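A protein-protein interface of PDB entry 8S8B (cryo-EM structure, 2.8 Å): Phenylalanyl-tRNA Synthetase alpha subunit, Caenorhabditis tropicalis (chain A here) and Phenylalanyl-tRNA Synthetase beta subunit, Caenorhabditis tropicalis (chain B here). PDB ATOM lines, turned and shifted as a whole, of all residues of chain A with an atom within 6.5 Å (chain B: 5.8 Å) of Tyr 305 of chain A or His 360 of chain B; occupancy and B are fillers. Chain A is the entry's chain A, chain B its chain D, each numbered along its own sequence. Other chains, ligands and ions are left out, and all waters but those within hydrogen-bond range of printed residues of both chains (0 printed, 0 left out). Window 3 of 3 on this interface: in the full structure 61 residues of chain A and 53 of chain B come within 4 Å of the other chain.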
ATOM      1  N   ARG A 295      25.847  31.375  -7.862  1.00  0.00           N
ATOM      2  CA  ARG A 295      25.590  30.195  -7.040  1.00  0.00           C
ATOM      3  C   ARG A 295      24.609  29.246  -7.720  1.00  0.00           C
ATOM      4  O   ARG A 295      24.777  28.021  -7.661  1.00  0.00           O
ATOM      5  CB  ARG A 295      25.075  30.610  -5.662  1.00  0.00           C
ATOM      6  CG  ARG A 295      26.133  31.227  -4.765  1.00  0.00           C
ATOM      7  CD  ARG A 295      25.630  31.383  -3.340  1.00  0.00           C
ATOM      8  NE  ARG A 295      24.497  32.296  -3.254  1.00  0.00           N
ATOM      9  CZ  ARG A 295      24.585  33.568  -2.892  1.00  0.00           C
ATOM     10  NH1 ARG A 295      25.743  34.113  -2.560  1.00  0.00           N
ATOM     11  NH2 ARG A 295      23.484  34.311  -2.860  1.00  0.00           N
ATOM     12  N   VAL A 299      25.388  25.343  -8.741  1.00  0.00           N
ATOM     13  CA  VAL A 299      24.619  24.187  -8.287  1.00  0.00           C
ATOM     14  C   VAL A 299      24.033  23.430  -9.474  1.00  0.00           C
ATOM     15  O   VAL A 299      23.873  22.205  -9.424  1.00  0.00           O
ATOM     16  CB  VAL A 299      23.532  24.604  -7.278  1.00  0.00           C
ATOM     17  CG1 VAL A 299      22.346  25.248  -7.970  1.00  0.00           C
ATOM     18  CG2 VAL A 299      23.084  23.402  -6.466  1.00  0.00           C
ATOM     19  N   GLY A 303      26.859  20.950  -8.890  1.00  0.00           N
ATOM     20  CA  GLY A 303      26.264  20.419  -7.683  1.00  0.00           C
ATOM     21  C   GLY A 303      26.874  21.005  -6.428  1.00  0.00           C
ATOM     22  O   GLY A 303      27.762  21.859  -6.500  1.00  0.00           O
ATOM     23  N   GLY A 304      26.414  20.545  -5.272  1.00  0.00           N
ATOM     24  CA  GLY A 304      26.874  21.081  -4.008  1.00  0.00           C
ATOM     25  C   GLY A 304      25.747  21.102  -3.001  1.00  0.00           C
ATOM     26  O   GLY A 304      24.601  20.763  -3.302  1.00  0.00           O
ATOM     27  N   TYR A 305      26.086  21.521  -1.782  1.00  0.00           N
ATOM     28  CA  TYR A 305      25.149  21.509  -0.660  1.00  0.00           C
ATOM     29  C   TYR A 305      24.594  20.105  -0.428  1.00  0.00           C
ATOM     30  O   TYR A 305      23.411  19.925  -0.139  1.00  0.00           O
ATOM     31  CB  TYR A 305      24.012  22.513  -0.868  1.00  0.00           C
ATOM     32  CG  TYR A 305      24.479  23.894  -1.257  1.00  0.00           C
ATOM     33  CD1 TYR A 305      25.070  24.735  -0.326  1.00  0.00           C
ATOM     34  CD2 TYR A 305      24.322  24.361  -2.554  1.00  0.00           C
ATOM     35  CE1 TYR A 305      25.498  25.998  -0.676  1.00  0.00           C
ATOM     36  CE2 TYR A 305      24.747  25.624  -2.913  1.00  0.00           C
ATOM     37  CZ  TYR A 305      25.334  26.437  -1.970  1.00  0.00           C
ATOM     38  OH  TYR A 305      25.759  27.698  -2.319  1.00  0.00           O
ATOM     39  N   GLY A 306      25.457  19.102  -0.564  1.00  0.00           N
ATOM     40  CA  GLY A 306      25.033  17.728  -0.394  1.00  0.00           C
ATOM     41  C   GLY A 306      24.230  17.161  -1.540  1.00  0.00           C
ATOM     42  O   GLY A 306      23.529  16.164  -1.356  1.00  0.00           O
ATOM     43  N   SER A 307      24.311  17.764  -2.719  1.00  0.00           N
ATOM     44  CA  SER A 307      23.583  17.318  -3.898  1.00  0.00           C
ATOM     45  C   SER A 307      24.560  16.839  -4.964  1.00  0.00           C
ATOM     46  O   SER A 307      25.781  16.930  -4.812  1.00  0.00           O
ATOM     47  CB  SER A 307      22.698  18.441  -4.444  1.00  0.00           C
ATOM     48  OG  SER A 307      22.065  18.046  -5.646  1.00  0.00           O
ATOM     49  N   ALA A 308      24.005  16.319  -6.060  1.00  0.00           N
ATOM     50  CA  ALA A 308      24.807  15.805  -7.159  1.00  0.00           C
ATOM     51  C   ALA A 308      24.687  16.615  -8.440  1.00  0.00           C
ATOM     52  O   ALA A 308      25.592  16.546  -9.276  1.00  0.00           O
ATOM     53  CB  ALA A 308      24.433  14.349  -7.462  1.00  0.00           C
ATOM     54  N   ARG A 438      12.544  21.739  -2.535  1.00  0.00           N
ATOM     55  CA  ARG A 438      13.820  21.056  -2.440  1.00  0.00           C
ATOM     56  C   ARG A 438      14.869  21.958  -1.792  1.00  0.00           C
ATOM     57  O   ARG A 438      14.838  23.178  -1.960  1.00  0.00           O
ATOM     58  CB  ARG A 438      14.301  20.628  -3.822  1.00  0.00           C
ATOM     59  CG  ARG A 438      13.321  19.765  -4.589  1.00  0.00           C
ATOM     60  CD  ARG A 438      13.900  19.344  -5.926  1.00  0.00           C
ATOM     61  NE  ARG A 438      15.149  18.609  -5.763  1.00  0.00           N
ATOM     62  CZ  ARG A 438      15.248  17.288  -5.779  1.00  0.00           C
ATOM     63  NH1 ARG A 438      14.191  16.517  -5.973  1.00  0.00           N
ATOM     64  NH2 ARG A 438      16.439  16.725  -5.597  1.00  0.00           N
ATOM     65  N   PRO A 439      15.812  21.378  -1.047  1.00  0.00           N
ATOM     66  CA  PRO A 439      16.902  22.189  -0.484  1.00  0.00           C
ATOM     67  C   PRO A 439      17.794  22.819  -1.535  1.00  0.00           C
ATOM     68  O   PRO A 439      18.503  23.782  -1.227  1.00  0.00           O
ATOM     69  CB  PRO A 439      17.680  21.183   0.374  1.00  0.00           C
ATOM     70  CG  PRO A 439      16.718  20.080   0.638  1.00  0.00           C
ATOM     71  CD  PRO A 439      15.871  19.984  -0.587  1.00  0.00           C
ATOM     72  N   GLU A 440      17.789  22.303  -2.764  1.00  0.00           N
ATOM     73  CA  GLU A 440      18.653  22.823  -3.814  1.00  0.00           C
ATOM     74  C   GLU A 440      18.166  24.146  -4.387  1.00  0.00           C
ATOM     75  O   GLU A 440      18.904  24.774  -5.151  1.00  0.00           O
ATOM     76  CB  GLU A 440      18.784  21.790  -4.929  1.00  0.00           C
ATOM     77  CG  GLU A 440      19.503  20.525  -4.502  1.00  0.00           C
ATOM     78  CD  GLU A 440      18.972  19.295  -5.202  1.00  0.00           C
ATOM     79  OE1 GLU A 440      17.737  19.152  -5.298  1.00  0.00           O
ATOM     80  OE2 GLU A 440      19.788  18.472  -5.661  1.00  0.00           O
ATOM     81  N   LEU A 443      18.901  26.711  -0.205  1.00  0.00           N
ATOM     82  CA  LEU A 443      20.220  27.036   0.332  1.00  0.00           C
ATOM     83  C   LEU A 443      20.967  28.085  -0.484  1.00  0.00           C
ATOM     84  O   LEU A 443      21.584  28.973   0.130  1.00  0.00           O
ATOM     85  CB  LEU A 443      21.047  25.753   0.476  1.00  0.00           C
ATOM     86  CG  LEU A 443      20.432  24.694   1.389  1.00  0.00           C
ATOM     87  CD1 LEU A 443      21.361  23.506   1.536  1.00  0.00           C
ATOM     88  CD2 LEU A 443      20.110  25.291   2.742  1.00  0.00           C
ATOM     89  N   PRO A 444      20.984  28.051  -1.822  1.00  0.00           N
ATOM     90  CA  PRO A 444      21.615  29.156  -2.559  1.00  0.00           C
ATOM     91  C   PRO A 444      20.995  30.515  -2.282  1.00  0.00           C
ATOM     92  O   PRO A 444      21.698  31.528  -2.368  1.00  0.00           O
ATOM     93  CB  PRO A 444      21.436  28.741  -4.023  1.00  0.00           C
ATOM     94  CG  PRO A 444      21.406  27.270  -3.975  1.00  0.00           C
ATOM     95  CD  PRO A 444      20.653  26.932  -2.724  1.00  0.00           C
ATOM     96  N   MET B 308      25.284   7.107  -0.272  1.00  0.00           N
ATOM     97  CA  MET B 308      24.898   8.331   0.413  1.00  0.00           C
ATOM     98  C   MET B 308      24.871   8.089   1.916  1.00  0.00           C
ATOM     99  O   MET B 308      24.786   6.953   2.387  1.00  0.00           O
ATOM    100  CB  MET B 308      23.527   8.829  -0.060  1.00  0.00           C
ATOM    101  CG  MET B 308      23.466   9.213  -1.521  1.00  0.00           C
ATOM    102  SD  MET B 308      21.860   9.903  -1.952  1.00  0.00           S
ATOM    103  CE  MET B 308      22.137  10.361  -3.656  1.00  0.00           C
ATOM    104  N   ILE B 358      17.783   9.824  -7.714  1.00  0.00           N
ATOM    105  CA  ILE B 358      18.140  10.084  -6.325  1.00  0.00           C
ATOM    106  C   ILE B 358      19.356  11.002  -6.346  1.00  0.00           C
ATOM    107  O   ILE B 358      20.486  10.551  -6.552  1.00  0.00           O
ATOM    108  CB  ILE B 358      18.421   8.791  -5.558  1.00  0.00           C
ATOM    109  CG1 ILE B 358      17.267   7.805  -5.727  1.00  0.00           C
ATOM    110  CG2 ILE B 358      18.647   9.085  -4.091  1.00  0.00           C
ATOM    111  CD1 ILE B 358      15.960   8.296  -5.171  1.00  0.00           C
ATOM    112  N   LEU B 359      19.128  12.295  -6.131  1.00  0.00           N
ATOM    113  CA  LEU B 359      20.193  13.288  -6.107  1.00  0.00           C
ATOM    114  C   LEU B 359      20.514  13.768  -4.699  1.00  0.00           C
ATOM    115  O   LEU B 359      21.685  13.827  -4.315  1.00  0.00           O
ATOM    116  CB  LEU B 359      19.813  14.485  -6.987  1.00  0.00           C
ATOM    117  CG  LEU B 359      19.492  14.170  -8.447  1.00  0.00           C
ATOM    118  CD1 LEU B 359      19.079  15.432  -9.182  1.00  0.00           C
ATOM    119  CD2 LEU B 359      20.683  13.520  -9.123  1.00  0.00           C
ATOM    120  N   HIS B 360      19.497  14.110  -3.919  1.00  0.00           N
ATOM    121  CA  HIS B 360      19.660  14.628  -2.571  1.00  0.00           C
ATOM    122  C   HIS B 360      19.049  13.657  -1.569  1.00  0.00           C
ATOM    123  O   HIS B 360      18.393  12.680  -1.937  1.00  0.00           O
ATOM    124  CB  HIS B 360      19.016  16.015  -2.446  1.00  0.00           C
ATOM    125  CG  HIS B 360      19.546  16.832  -1.310  1.00  0.00           C
ATOM    126  ND1 HIS B 360      20.697  16.502  -0.629  1.00  0.00           N
ATOM    127  CD2 HIS B 360      19.083  17.968  -0.739  1.00  0.00           C
ATOM    128  CE1 HIS B 360      20.919  17.399   0.315  1.00  0.00           C
ATOM    129  NE2 HIS B 360      19.954  18.299   0.270  1.00  0.00           N
ATOM    130  N   ALA B 361      19.274  13.933  -0.284  1.00  0.00           N
ATOM    131  CA  ALA B 361      18.691  13.105   0.765  1.00  0.00           C
ATOM    132  C   ALA B 361      17.173  13.208   0.809  1.00  0.00           C
ATOM    133  O   ALA B 361      16.511  12.260   1.251  1.00  0.00           O
ATOM    134  CB  ALA B 361      19.279  13.484   2.123  1.00  0.00           C
ATOM    135  N   CYS B 362      16.603  14.326   0.355  1.00  0.00           N
ATOM    136  CA  CYS B 362      15.153  14.464   0.352  1.00  0.00           C
ATOM    137  C   CYS B 362      14.475  13.400  -0.499  1.00  0.00           C
ATOM    138  O   CYS B 362      13.372  12.961  -0.154  1.00  0.00           O
ATOM    139  CB  CYS B 362      14.754  15.858  -0.132  1.00  0.00           C
ATOM    140  SG  CYS B 362      15.261  16.260  -1.814  1.00  0.00           S
ATOM    141  N   ASP B 363      15.111  12.962  -1.587  1.00  0.00           N
ATOM    142  CA  ASP B 363      14.566  11.855  -2.362  1.00  0.00           C
ATOM    143  C   ASP B 363      14.455  10.596  -1.515  1.00  0.00           C
ATOM    144  O   ASP B 363      13.445   9.882  -1.586  1.00  0.00           O
ATOM    145  CB  ASP B 363      15.436  11.596  -3.590  1.00  0.00           C
ATOM    146  CG  ASP B 363      15.608  12.830  -4.452  1.00  0.00           C
ATOM    147  OD1 ASP B 363      14.657  13.629  -4.546  1.00  0.00           O
ATOM    148  OD2 ASP B 363      16.699  13.005  -5.033  1.00  0.00           O
ATOM    149  N   ILE B 364      15.467  10.317  -0.695  1.00  0.00           N
ATOM    150  CA  ILE B 364      15.361   9.198   0.228  1.00  0.00           C
ATOM    151  C   ILE B 364      14.218   9.426   1.206  1.00  0.00           C
ATOM    152  O   ILE B 364      13.478   8.488   1.530  1.00  0.00           O
ATOM    153  CB  ILE B 364      16.697   8.971   0.953  1.00  0.00           C
ATOM    154  CG1 ILE B 364      17.787   8.618  -0.059  1.00  0.00           C
ATOM    155  CG2 ILE B 364      16.563   7.869   1.981  1.00  0.00           C
ATOM    156  CD1 ILE B 364      19.124   8.306   0.566  1.00  0.00           C
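His 360 of chain B touches Tyr 305 of chain A. Leu 359 of chain B touches Ser 307 of chain A. Leu 359 of chain B touches Ala 308 of chain A (O to N, 3.8 Å). Arg 438 of chain A touches Cys 362 of chain B (NH2 to SG, 3.99 Å). Pro 439 of chain A touches His 360 of chain B. Cys 362 of chain B touches Pro 439 of chain A.
A ring nitrogen (ND1) of His 360 of chain B sits at hydrogen-bond distance from the backbone carbonyl oxygen of Gly 306 of chain A, at 2.9 Å. The side-chain carboxylate of Asp 363 of chain B lies within salt-bridge range of the guanidinium group of Arg 438 of chain A, 3.3 Å away.
Printed residues of chain B that touch a printed residue of chain A: Leu 359, His 360, Cys 362 and Asp 363. Of the 13 printed residues of chain A, 6 touch a printed residue of chain B. Printed residues of chain A that touch a printed residue of chain B: Tyr 305, Gly 306, Ser 307, Ala 308, Arg 438 and Pro 439. Hydrophobic or aromatic side chains of chain A within 4 Å of the printed part of chain B: Pro 439. Among the printed residues, 8 pairs touch across the chains. Among the printed residues, Asp or Glu carboxylates within 4 Å of a Lys or Arg side-chain nitrogen of the other chain: Arg 438 of chain A with Asp 363 of chain B (3.3 Å).
NE of Arg 438 of chain A lies within salt-bridge range of OE1 of Glu 440 of chain A, 2.7 Å away. The backbone NH (N) of Leu 359 of chain B sits at hydrogen-bond distance from the side-chain carboxylate (OD2) of Asp 363 of chain B, at 2.8 Å. N of His 360 of chain B lies within hydrogen-bond range of OD2 of Asp 363 of chain B.
Of the printed residues of chain B, Tyr 305 of chain A touches His 360 (3.6 Å). Printed residues of chain B within 4 Å of Gly 306 of chain A: His 360. Of the printed residues of chain B, Arg 438 of chain A touches Cys 362 (3.99 Å) and Asp 363 (3.3 Å).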
